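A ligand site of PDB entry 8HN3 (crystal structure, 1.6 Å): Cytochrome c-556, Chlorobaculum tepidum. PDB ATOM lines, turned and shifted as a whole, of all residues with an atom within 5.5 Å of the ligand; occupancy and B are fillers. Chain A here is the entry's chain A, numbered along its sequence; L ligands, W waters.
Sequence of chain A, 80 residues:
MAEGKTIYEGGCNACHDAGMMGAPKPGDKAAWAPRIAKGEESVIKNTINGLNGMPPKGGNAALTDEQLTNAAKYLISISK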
ATOM      1  N   ILE A   7       8.342   8.441   5.614  1.00  0.00           N
ATOM      2  CA  ILE A   7       9.778   8.635   5.224  1.00  0.00           C
ATOM      3  C   ILE A   7       9.957   9.745   4.208  1.00  0.00           C
ATOM      4  O   ILE A   7      10.764  10.675   4.359  1.00  0.00           O
ATOM      5  CB  ILE A   7      10.384   7.381   4.738  1.00  0.00           C
ATOM      6  CG1 ILE A   7      10.577   6.447   5.970  1.00  0.00           C
ATOM      7  CG2 ILE A   7      11.787   7.573   4.028  1.00  0.00           C
ATOM      8  CD1 ILE A   7      10.635   5.099   5.421  1.00  0.00           C
ATOM      9  N   TYR A   8       9.070   9.665   3.202  1.00  0.00           N
ATOM     10  CA  TYR A   8       9.054  10.762   2.180  1.00  0.00           C
ATOM     11  C   TYR A   8       8.934  12.185   2.782  1.00  0.00           C
ATOM     12  O   TYR A   8       9.618  13.134   2.310  1.00  0.00           O
ATOM     13  CB  TYR A   8       7.979  10.530   1.077  1.00  0.00           C
ATOM     14  CG  TYR A   8       7.986  11.578   0.066  1.00  0.00           C
ATOM     15  CD1 TYR A   8       8.941  11.589  -0.898  1.00  0.00           C
ATOM     16  CD2 TYR A   8       7.058  12.541   0.084  1.00  0.00           C
ATOM     17  CE1 TYR A   8       9.076  12.608  -1.806  1.00  0.00           C
ATOM     18  CE2 TYR A   8       7.139  13.598  -0.849  1.00  0.00           C
ATOM     19  CZ  TYR A   8       8.148  13.581  -1.789  1.00  0.00           C
ATOM     20  OH  TYR A   8       8.310  14.629  -2.724  1.00  0.00           O
ATOM     21  N   GLY A  11      12.235  14.353   4.566  1.00  0.00           N
ATOM     22  CA  GLY A  11      13.363  14.904   3.967  1.00  0.00           C
ATOM     23  C   GLY A  11      13.487  14.700   2.460  1.00  0.00           C
ATOM     24  O   GLY A  11      13.954  15.575   1.776  1.00  0.00           O
ATOM     25  N   CYS A  12      13.004  13.573   1.999  1.00  0.00           N
ATOM     26  CA  CYS A  12      13.045  13.283   0.544  1.00  0.00           C
ATOM     27  C   CYS A  12      12.334  14.395  -0.211  1.00  0.00           C
ATOM     28  O   CYS A  12      12.718  14.806  -1.324  1.00  0.00           O
ATOM     29  CB  CYS A  12      12.309  11.985   0.215  1.00  0.00           C
ATOM     30  SG  CYS A  12      12.713  10.534   1.259  1.00  0.00           S
ATOM     31  N   CYS A  15      13.846  17.771  -1.896  1.00  0.00           N
ATOM     32  CA  CYS A  15      14.214  17.873  -3.282  1.00  0.00           C
ATOM     33  C   CYS A  15      13.028  17.537  -4.192  1.00  0.00           C
ATOM     34  O   CYS A  15      12.901  18.155  -5.271  1.00  0.00           O
ATOM     35  CB  CYS A  15      15.333  16.868  -3.551  1.00  0.00           C
ATOM     36  SG  CYS A  15      16.861  17.336  -2.782  1.00  0.00           S
ATOM     37  N   HIS A  16      12.279  16.492  -3.873  1.00  0.00           N
ATOM     38  CA  HIS A  16      11.265  15.988  -4.785  1.00  0.00           C
ATOM     39  C   HIS A  16      10.045  16.891  -4.937  1.00  0.00           C
ATOM     40  O   HIS A  16       9.508  16.988  -6.038  1.00  0.00           O
ATOM     41  CB  HIS A  16      10.863  14.519  -4.440  1.00  0.00           C
ATOM     42  CG  HIS A  16      11.926  13.548  -4.867  1.00  0.00           C
ATOM     43  ND1 HIS A  16      11.842  12.936  -6.096  1.00  0.00           N
ATOM     44  CD2 HIS A  16      13.039  13.080  -4.262  1.00  0.00           C
ATOM     45  CE1 HIS A  16      12.857  12.116  -6.204  1.00  0.00           C
ATOM     46  NE2 HIS A  16      13.641  12.209  -5.142  1.00  0.00           N
ATOM     47  N   MET A  20      14.047  19.705  -7.489  1.00  0.00           N
ATOM     48  CA  MET A  20      15.421  20.193  -7.521  1.00  0.00           C
ATOM     49  C   MET A  20      16.240  19.262  -8.440  1.00  0.00           C
ATOM     50  O   MET A  20      16.193  18.071  -8.284  1.00  0.00           O
ATOM     51  CB  MET A  20      16.008  20.196  -6.121  1.00  0.00           C
ATOM     52  CG  MET A  20      17.174  21.023  -5.948  1.00  0.00           C
ATOM     53  SD  MET A  20      17.843  20.877  -4.232  1.00  0.00           S
ATOM     54  CE  MET A  20      16.229  21.429  -3.581  1.00  0.00           C
ATOM     55  N   MET A  21      17.034  19.885  -9.286  1.00  0.00           N
ATOM     56  CA  MET A  21      17.980  19.149 -10.175  1.00  0.00           C
ATOM     57  C   MET A  21      17.268  18.291 -11.153  1.00  0.00           C
ATOM     58  O   MET A  21      17.904  17.505 -11.894  1.00  0.00           O
ATOM     59  CB  MET A  21      19.027  18.333  -9.412  1.00  0.00           C
ATOM     60  CG  MET A  21      19.938  19.126  -8.511  1.00  0.00           C
ATOM     61  SD  MET A  21      20.994  18.158  -7.450  1.00  0.00           S
ATOM     62  CE  MET A  21      19.760  17.719  -6.204  1.00  0.00           C
ATOM     63  N   GLY A  22      15.989  18.420 -11.290  1.00  0.00           N
ATOM     64  CA  GLY A  22      15.201  17.505 -12.117  1.00  0.00           C
ATOM     65  C   GLY A  22      14.668  16.280 -11.408  1.00  0.00           C
ATOM     66  O   GLY A  22      14.219  15.340 -12.025  1.00  0.00           O
ATOM     67  N   ALA A  23      14.707  16.299 -10.072  1.00  0.00           N
ATOM     68  CA  ALA A  23      14.114  15.211  -9.296  1.00  0.00           C
ATOM     69  C   ALA A  23      12.638  15.071  -9.699  1.00  0.00           C
ATOM     70  O   ALA A  23      11.910  16.073  -9.820  1.00  0.00           O
ATOM     71  CB  ALA A  23      14.162  15.492  -7.845  1.00  0.00           C
ATOM     72  N   PRO A  24      12.142  13.842  -9.862  1.00  0.00           N
ATOM     73  CA  PRO A  24      10.757  13.663 -10.266  1.00  0.00           C
ATOM     74  C   PRO A  24       9.801  13.960  -9.128  1.00  0.00           C
ATOM     75  O   PRO A  24       9.864  13.417  -8.005  1.00  0.00           O
ATOM     76  CB  PRO A  24      10.725  12.175 -10.684  1.00  0.00           C
ATOM     77  CG  PRO A  24      11.838  11.514  -9.896  1.00  0.00           C
ATOM     78  CD  PRO A  24      12.936  12.565  -9.887  1.00  0.00           C
ATOM     79  N   TRP A  32       7.441  10.239 -14.021  1.00  0.00           N
ATOM     80  CA  TRP A  32       7.624   8.920 -13.452  1.00  0.00           C
ATOM     81  C   TRP A  32       7.489   7.788 -14.438  1.00  0.00           C
ATOM     82  O   TRP A  32       8.068   6.725 -14.297  1.00  0.00           O
ATOM     83  CB  TRP A  32       6.716   8.691 -12.260  1.00  0.00           C
ATOM     84  CG  TRP A  32       7.203   9.364 -10.982  1.00  0.00           C
ATOM     85  CD1 TRP A  32       6.904  10.629 -10.538  1.00  0.00           C
ATOM     86  CD2 TRP A  32       8.200   8.860 -10.099  1.00  0.00           C
ATOM     87  NE1 TRP A  32       7.617  10.917  -9.422  1.00  0.00           N
ATOM     88  CE2 TRP A  32       8.426   9.843  -9.114  1.00  0.00           C
ATOM     89  CE3 TRP A  32       8.891   7.653 -10.013  1.00  0.00           C
ATOM     90  CZ2 TRP A  32       9.413   9.712  -8.114  1.00  0.00           C
ATOM     91  CZ3 TRP A  32       9.773   7.524  -8.976  1.00  0.00           C
ATOM     92  CH2 TRP A  32      10.041   8.523  -8.039  1.00  0.00           C
ATOM     93  N   ARG A  35      10.597   6.110 -15.725  1.00  0.00           N
ATOM     94  CA  ARG A  35      11.363   5.548 -14.585  1.00  0.00           C
ATOM     95  C   ARG A  35      10.699   4.208 -14.108  1.00  0.00           C
ATOM     96  O   ARG A  35      11.486   3.293 -13.812  1.00  0.00           O
ATOM     97  CB  ARG A  35      11.396   6.565 -13.418  1.00  0.00           C
ATOM     98  CG  ARG A  35      12.075   7.844 -13.800  1.00  0.00           C
ATOM     99  CD  ARG A  35      12.082   8.848 -12.668  1.00  0.00           C
ATOM    100  NE  ARG A  35      12.724  10.128 -13.033  1.00  0.00           N
ATOM    101  CZ  ARG A  35      13.994  10.404 -12.956  1.00  0.00           C
ATOM    102  NH1 ARG A  35      14.877   9.607 -12.392  1.00  0.00           N
ATOM    103  NH2 ARG A  35      14.416  11.591 -13.418  1.00  0.00           N
ATOM    104  N   SER A  42      14.948  -1.683 -10.604  1.00  0.00           N
ATOM    105  CA  SER A  42      15.866  -0.669 -10.949  1.00  0.00           C
ATOM    106  C   SER A  42      15.640   0.673 -10.127  1.00  0.00           C
ATOM    107  O   SER A  42      16.613   1.290  -9.708  1.00  0.00           O
ATOM    108  CB  SER A  42      15.995  -0.329 -12.440  1.00  0.00           C
ATOM    109  OG  SER A  42      14.898   0.463 -12.825  1.00  0.00           O
ATOM    110  N   VAL A  43      14.403   0.964  -9.951  1.00  0.00           N
ATOM    111  CA  VAL A  43      14.029   2.181  -9.164  1.00  0.00           C
ATOM    112  C   VAL A  43      14.534   2.057  -7.708  1.00  0.00           C
ATOM    113  O   VAL A  43      15.177   2.965  -7.140  1.00  0.00           O
ATOM    114  CB  VAL A  43      12.507   2.489  -9.176  1.00  0.00           C
ATOM    115  CG1 VAL A  43      12.203   3.687  -8.276  1.00  0.00           C
ATOM    116  CG2 VAL A  43      12.070   2.718 -10.593  1.00  0.00           C
ATOM    117  N   ASN A  46      18.315   2.325  -7.466  1.00  0.00           N
ATOM    118  CA  ASN A  46      18.753   3.691  -7.531  1.00  0.00           C
ATOM    119  C   ASN A  46      18.439   4.483  -6.253  1.00  0.00           C
ATOM    120  O   ASN A  46      19.237   5.411  -5.918  1.00  0.00           O
ATOM    121  CB  ASN A  46      18.092   4.411  -8.715  1.00  0.00           C
ATOM    122  CG  ASN A  46      18.669   3.908 -10.054  1.00  0.00           C
ATOM    123  OD1 ASN A  46      19.801   3.495 -10.130  1.00  0.00           O
ATOM    124  ND2 ASN A  46      17.831   4.009 -11.076  1.00  0.00           N
ATOM    125  N   THR A  47      17.407   4.123  -5.568  1.00  0.00           N
ATOM    126  CA  THR A  47      17.055   4.786  -4.271  1.00  0.00           C
ATOM    127  C   THR A  47      18.099   4.475  -3.171  1.00  0.00           C
ATOM    128  O   THR A  47      18.577   5.306  -2.437  1.00  0.00           O
ATOM    129  CB  THR A  47      15.700   4.362  -3.882  1.00  0.00           C
ATOM    130  OG1 THR A  47      14.682   4.592  -4.887  1.00  0.00           O
ATOM    131  CG2 THR A  47      15.205   5.072  -2.597  1.00  0.00           C
ATOM    132  N   LEU A  51      21.680   7.885  -7.597  1.00  0.00           N
ATOM    133  CA  LEU A  51      21.728   8.035  -9.076  1.00  0.00           C
ATOM    134  C   LEU A  51      21.960   9.575  -9.287  1.00  0.00           C
ATOM    135  O   LEU A  51      21.042  10.341  -9.027  1.00  0.00           O
ATOM    136  CB  LEU A  51      20.482   7.611  -9.744  1.00  0.00           C
ATOM    137  CG  LEU A  51      20.353   7.875 -11.256  1.00  0.00           C
ATOM    138  CD1 LEU A  51      21.403   7.134 -12.009  1.00  0.00           C
ATOM    139  CD2 LEU A  51      18.994   7.493 -11.685  1.00  0.00           C
ATOM    140  N   ASN A  52      23.135   9.975  -9.787  1.00  0.00           N
ATOM    141  CA  ASN A  52      23.319  11.374 -10.098  1.00  0.00           C
ATOM    142  C   ASN A  52      23.011  12.258  -8.912  1.00  0.00           C
ATOM    143  O   ASN A  52      23.621  11.997  -7.857  1.00  0.00           O
ATOM    144  CB  ASN A  52      22.502  11.753 -11.365  1.00  0.00           C
ATOM    145  CG  ASN A  52      22.990  11.061 -12.569  1.00  0.00           C
ATOM    146  OD1 ASN A  52      24.186  10.789 -12.751  1.00  0.00           O
ATOM    147  ND2 ASN A  52      22.093  10.877 -13.512  1.00  0.00           N
ATOM    148  N   GLY A  53      22.108  13.203  -8.988  1.00  0.00           N
ATOM    149  CA  GLY A  53      21.811  14.112  -7.858  1.00  0.00           C
ATOM    150  C   GLY A  53      20.970  13.448  -6.807  1.00  0.00           C
ATOM    151  O   GLY A  53      20.752  14.120  -5.747  1.00  0.00           O
ATOM    152  N   MET A  54      20.457  12.245  -7.010  1.00  0.00           N
ATOM    153  CA  MET A  54      19.722  11.479  -5.998  1.00  0.00           C
ATOM    154  C   MET A  54      20.736  10.799  -5.070  1.00  0.00           C
ATOM    155  O   MET A  54      21.483   9.923  -5.505  1.00  0.00           O
ATOM    156  CB  MET A  54      18.933  10.424  -6.709  1.00  0.00           C
ATOM    157  CG  MET A  54      18.197   9.425  -5.816  1.00  0.00           C
ATOM    158  SD  MET A  54      17.395  10.077  -4.362  1.00  0.00           S
ATOM    159  CE  MET A  54      17.034   8.495  -3.525  1.00  0.00           C
ATOM    160  N   PRO A  55      20.907  11.240  -3.859  1.00  0.00           N
ATOM    161  CA  PRO A  55      21.944  10.686  -2.978  1.00  0.00           C
ATOM    162  C   PRO A  55      21.607   9.276  -2.548  1.00  0.00           C
ATOM    163  O   PRO A  55      20.433   8.916  -2.470  1.00  0.00           O
ATOM    164  CB  PRO A  55      21.931  11.611  -1.723  1.00  0.00           C
ATOM    165  CG  PRO A  55      21.023  12.720  -2.079  1.00  0.00           C
ATOM    166  CD  PRO A  55      20.059  12.268  -3.178  1.00  0.00           C
ATOM    167  N   LYS A  57      20.401   6.525  -0.375  1.00  0.00           N
ATOM    168  CA  LYS A  57      19.471   6.489   0.740  1.00  0.00           C
ATOM    169  C   LYS A  57      18.808   7.826   0.942  1.00  0.00           C
ATOM    170  O   LYS A  57      18.274   8.112   2.001  1.00  0.00           O
ATOM    171  CB  LYS A  57      20.167   6.019   2.006  1.00  0.00           C
ATOM    172  CG  LYS A  57      21.032   4.815   1.798  1.00  0.00           C
ATOM    173  CD  LYS A  57      21.348   4.107   3.160  1.00  0.00           C
ATOM    174  CE  LYS A  57      22.336   2.940   2.897  1.00  0.00           C
ATOM    175  NZ  LYS A  57      22.585   2.081   4.163  1.00  0.00           N
ATOM    176  N   GLY A  58      18.793   8.646  -0.134  1.00  0.00           N
ATOM    177  CA  GLY A  58      18.254  10.016   0.084  1.00  0.00           C
ATOM    178  C   GLY A  58      19.012  10.832   1.039  1.00  0.00           C
ATOM    179  O   GLY A  58      18.568  11.912   1.464  1.00  0.00           O
ATOM    180  N   GLY A  59      20.186  10.448   1.462  1.00  0.00           N
ATOM    181  CA  GLY A  59      21.006  11.061   2.488  1.00  0.00           C
ATOM    182  C   GLY A  59      20.444  10.830   3.928  1.00  0.00           C
ATOM    183  O   GLY A  59      20.953  11.439   4.853  1.00  0.00           O
ATOM    184  N   ASN A  60      19.534   9.867   4.073  1.00  0.00           N
ATOM    185  CA  ASN A  60      18.968   9.498   5.435  1.00  0.00           C
ATOM    186  C   ASN A  60      19.671   8.180   5.836  1.00  0.00           C
ATOM    187  O   ASN A  60      19.240   7.112   5.453  1.00  0.00           O
ATOM    188  CB  ASN A  60      17.495   9.415   5.413  1.00  0.00           C
ATOM    189  CG  ASN A  60      16.874   9.249   6.806  1.00  0.00           C
ATOM    190  OD1 ASN A  60      17.630   8.875   7.705  1.00  0.00           O
ATOM    191  ND2 ASN A  60      15.585   9.372   6.916  1.00  0.00           N
ATOM    192  N   LEU A  63      18.038   4.798   7.461  1.00  0.00           N
ATOM    193  CA  LEU A  63      17.002   3.980   6.848  1.00  0.00           C
ATOM    194  C   LEU A  63      17.505   2.609   6.411  1.00  0.00           C
ATOM    195  O   LEU A  63      18.639   2.491   5.857  1.00  0.00           O
ATOM    196  CB  LEU A  63      16.479   4.684   5.581  1.00  0.00           C
ATOM    197  CG  LEU A  63      15.785   5.992   5.903  1.00  0.00           C
ATOM    198  CD1 LEU A  63      15.303   6.621   4.577  1.00  0.00           C
ATOM    199  CD2 LEU A  63      14.611   5.858   6.774  1.00  0.00           C
ATOM    200  N   LEU A  68      13.596   2.223   2.464  1.00  0.00           N
ATOM    201  CA  LEU A  68      13.864   2.902   1.140  1.00  0.00           C
ATOM    202  C   LEU A  68      13.007   2.345   0.075  1.00  0.00           C
ATOM    203  O   LEU A  68      12.438   3.093  -0.740  1.00  0.00           O
ATOM    204  CB  LEU A  68      15.325   2.834   0.843  1.00  0.00           C
ATOM    205  CG  LEU A  68      16.204   3.676   1.734  1.00  0.00           C
ATOM    206  CD1 LEU A  68      17.644   3.245   1.742  1.00  0.00           C
ATOM    207  CD2 LEU A  68      16.081   5.174   1.342  1.00  0.00           C
ATOM    208  N   ALA A  71       9.503   3.670   0.566  1.00  0.00           N
ATOM    209  CA  ALA A  71       9.384   5.104   0.139  1.00  0.00           C
ATOM    210  C   ALA A  71       9.394   5.127  -1.393  1.00  0.00           C
ATOM    211  O   ALA A  71       8.554   5.906  -1.942  1.00  0.00           O
ATOM    212  CB  ALA A  71      10.553   5.837   0.697  1.00  0.00           C
ATOM    213  N   ALA A  72      10.233   4.360  -2.068  1.00  0.00           N
ATOM    214  CA  ALA A  72      10.172   4.368  -3.535  1.00  0.00           C
ATOM    215  C   ALA A  72       8.843   3.870  -4.029  1.00  0.00           C
ATOM    216  O   ALA A  72       8.248   4.411  -4.992  1.00  0.00           O
ATOM    217  CB  ALA A  72      11.265   3.506  -4.090  1.00  0.00           C
ATOM    218  N   LEU A  75       6.193   6.519  -3.780  1.00  0.00           N
ATOM    219  CA  LEU A  75       6.271   7.496  -4.908  1.00  0.00           C
ATOM    220  C   LEU A  75       5.706   6.864  -6.168  1.00  0.00           C
ATOM    221  O   LEU A  75       4.951   7.613  -6.941  1.00  0.00           O
ATOM    222  CB  LEU A  75       7.719   7.980  -5.105  1.00  0.00           C
ATOM    223  CG  LEU A  75       8.112   8.933  -4.032  1.00  0.00           C
ATOM    224  CD1 LEU A  75       9.590   9.158  -4.106  1.00  0.00           C
ATOM    225  CD2 LEU A  75       7.455  10.302  -4.221  1.00  0.00           C
HETATM  226 FE1  LIG L   1      15.389  11.176  -4.861  1.00  0.00          FE
HETATM  227  C1  LIG L   1      15.368  10.289  -8.213  1.00  0.00           C
HETATM  228  C2  LIG L   1      13.419   8.497  -4.116  1.00  0.00           C
HETATM  229  C3  LIG L   1      15.707  11.893  -1.542  1.00  0.00           C
HETATM  230  C4  LIG L   1      17.073  14.010  -5.615  1.00  0.00           C
HETATM  231  N1  LIG L   1      14.629   9.684  -5.942  1.00  0.00           N
HETATM  232  C5  LIG L   1      14.712   9.467  -7.269  1.00  0.00           C
HETATM  233  C6  LIG L   1      13.948   8.264  -7.644  1.00  0.00           C
HETATM  234  C7  LIG L   1      13.365   7.783  -6.512  1.00  0.00           C
HETATM  235  C8  LIG L   1      13.811   8.702  -5.485  1.00  0.00           C
HETATM  236  C9  LIG L   1      12.477   6.610  -6.350  1.00  0.00           C
HETATM  237  C10 LIG L   1      13.872   7.703  -9.073  1.00  0.00           C
HETATM  238  C11 LIG L   1      15.044   6.791  -9.330  1.00  0.00           C
HETATM  239  C12 LIG L   1      14.935   6.143 -10.715  1.00  0.00           C
HETATM  240  O1  LIG L   1      15.071   4.885 -10.857  1.00  0.00           O
HETATM  241  O2  LIG L   1      14.684   6.853 -11.751  1.00  0.00           O
HETATM  242  N2  LIG L   1      14.704  10.385  -3.172  1.00  0.00           N
HETATM  243  C13 LIG L   1      13.894   9.286  -3.092  1.00  0.00           C
HETATM  244  C14 LIG L   1      13.557   8.934  -1.697  1.00  0.00           C
HETATM  245  C15 LIG L   1      14.323   9.892  -0.941  1.00  0.00           C
HETATM  246  C16 LIG L   1      14.976  10.793  -1.903  1.00  0.00           C
HETATM  247  C17 LIG L   1      12.716   7.815  -1.192  1.00  0.00           C
HETATM  248  C18 LIG L   1      14.396  10.076   0.536  1.00  0.00           C
HETATM  249  C19 LIG L   1      14.589   8.881   1.345  1.00  0.00           C
HETATM  250  N3  LIG L   1      16.145  12.695  -3.803  1.00  0.00           N
HETATM  251  C20 LIG L   1      16.253  12.805  -2.477  1.00  0.00           C
HETATM  252  C21 LIG L   1      16.949  13.944  -2.023  1.00  0.00           C
HETATM  253  C22 LIG L   1      17.334  14.630  -3.193  1.00  0.00           C
HETATM  254  C23 LIG L   1      16.783  13.766  -4.249  1.00  0.00           C
HETATM  255  C24 LIG L   1      17.125  14.449  -0.666  1.00  0.00           C
HETATM  256  C25 LIG L   1      17.980  15.918  -3.469  1.00  0.00           C
HETATM  257  C26 LIG L   1      19.174  16.135  -2.752  1.00  0.00           C
HETATM  258  N4  LIG L   1      16.046  12.013  -6.591  1.00  0.00           N
HETATM  259  C27 LIG L   1      16.739  13.137  -6.705  1.00  0.00           C
HETATM  260  C28 LIG L   1      17.080  13.451  -8.076  1.00  0.00           C
HETATM  261  C29 LIG L   1      16.574  12.380  -8.793  1.00  0.00           C
HETATM  262  C30 LIG L   1      15.932  11.480  -7.823  1.00  0.00           C
HETATM  263  C31 LIG L   1      17.804  14.646  -8.610  1.00  0.00           C
HETATM  264  C32 LIG L   1      16.712  12.138 -10.279  1.00  0.00           C
HETATM  265  C33 LIG L   1      18.050  11.435 -10.574  1.00  0.00           C
HETATM  266  C34 LIG L   1      18.344  11.362 -12.103  1.00  0.00           C
HETATM  267  O3  LIG L   1      17.507  10.814 -12.867  1.00  0.00           O
HETATM  268  O4  LIG L   1      19.410  11.824 -12.468  1.00  0.00           O
HETATM  269  O   HOH W   1      16.057  12.604   2.026  1.00  0.00           O
HETATM  270  O   HOH W   2      20.408  14.104 -11.056  1.00  0.00           O
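SG of Cys 15 is covalently linked to C25 of the ligand (1.9 Å). The side-chain sulfur (SG) of Cys 12 is covalently linked to a carbon (C18) of the ligand (1.9 Å). NH1 of Arg 35 is in salt-bridge range of O2 of the ligand, 2.8 Å away. O4 of the ligand lies within hydrogen-bond range of ND2 of Asn 52, 3.0 Å away. A ring nitrogen (NE2) of His 16 is bound to an iron atom (FE1) of the ligand (2.0 Å). The side-chain amide nitrogen of Asn 46 is in hydrogen-bond range of an oxygen (O1) of the ligand, at 2.9 Å. An iron atom (FE1) of the ligand is bound by the side-chain sulfur (SD) of Met 54.
The backbone NH of Lys 57 lies within hydrogen-bond range of the backbone carbonyl oxygen of Thr 47. The side-chain amide nitrogen (ND2) of Asn 46 sits at hydrogen-bond distance from the backbone carbonyl oxygen (O) of Ser 42. The backbone carbonyl oxygen of Val 43 is in hydrogen-bond range of the side-chain hydroxyl of Thr 47, at 2.8 Å. ND1 of His 16 lies within hydrogen-bond range of O of Pro 24. N of Met 20 sits at hydrogen-bond distance from O of Cys 15.
Water W2 lies within hydrogen-bond range of N of Gly 53 (2.8 Å) and O4 of the ligand (2.9 Å). Water W1 lies within hydrogen-bond range of the backbone carbonyl oxygen (O) of Gly 58 (2.7 Å) and the backbone NH (N) of Cys 12 (3.2 Å).
Merely in contact with the ligand: Met 20 (3.8 Å), Met 21 (3.7 Å), Ala 23 (3.6 Å), Pro 24 (3.7 Å), Trp 32 (3.5 Å), Val 43 (3.4 Å), Thr 47 (3.3 Å), Leu 51 (3.5 Å), Gly 53 (3.7 Å), Pro 55 (3.6 Å), Lys 57 (3.8 Å), Gly 58 (3.6 Å), Leu 68 (3.996 Å), Ala 71 (3.5 Å) and Leu 75 (3.9 Å). Hydrophobic or aromatic side chains within 4 Å of the ligand: His 16, Met 21, Ala 23, Pro 24, Trp 32, Val 43, Leu 51, Met 54, Pro 55, Leu 68, Ala 71 and Leu 75. 22 residues have an atom within 4 Å of the ligand: Cys 12, Cys 15, His 16, Met 20, Met 21, Ala 23, Pro 24, Trp 32, Arg 35, Val 43, Asn 46, Thr 47, Leu 51, Asn 52, Gly 53, Met 54, Pro 55, Lys 57, Gly 58, Leu 68, Ala 71 and Leu 75.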
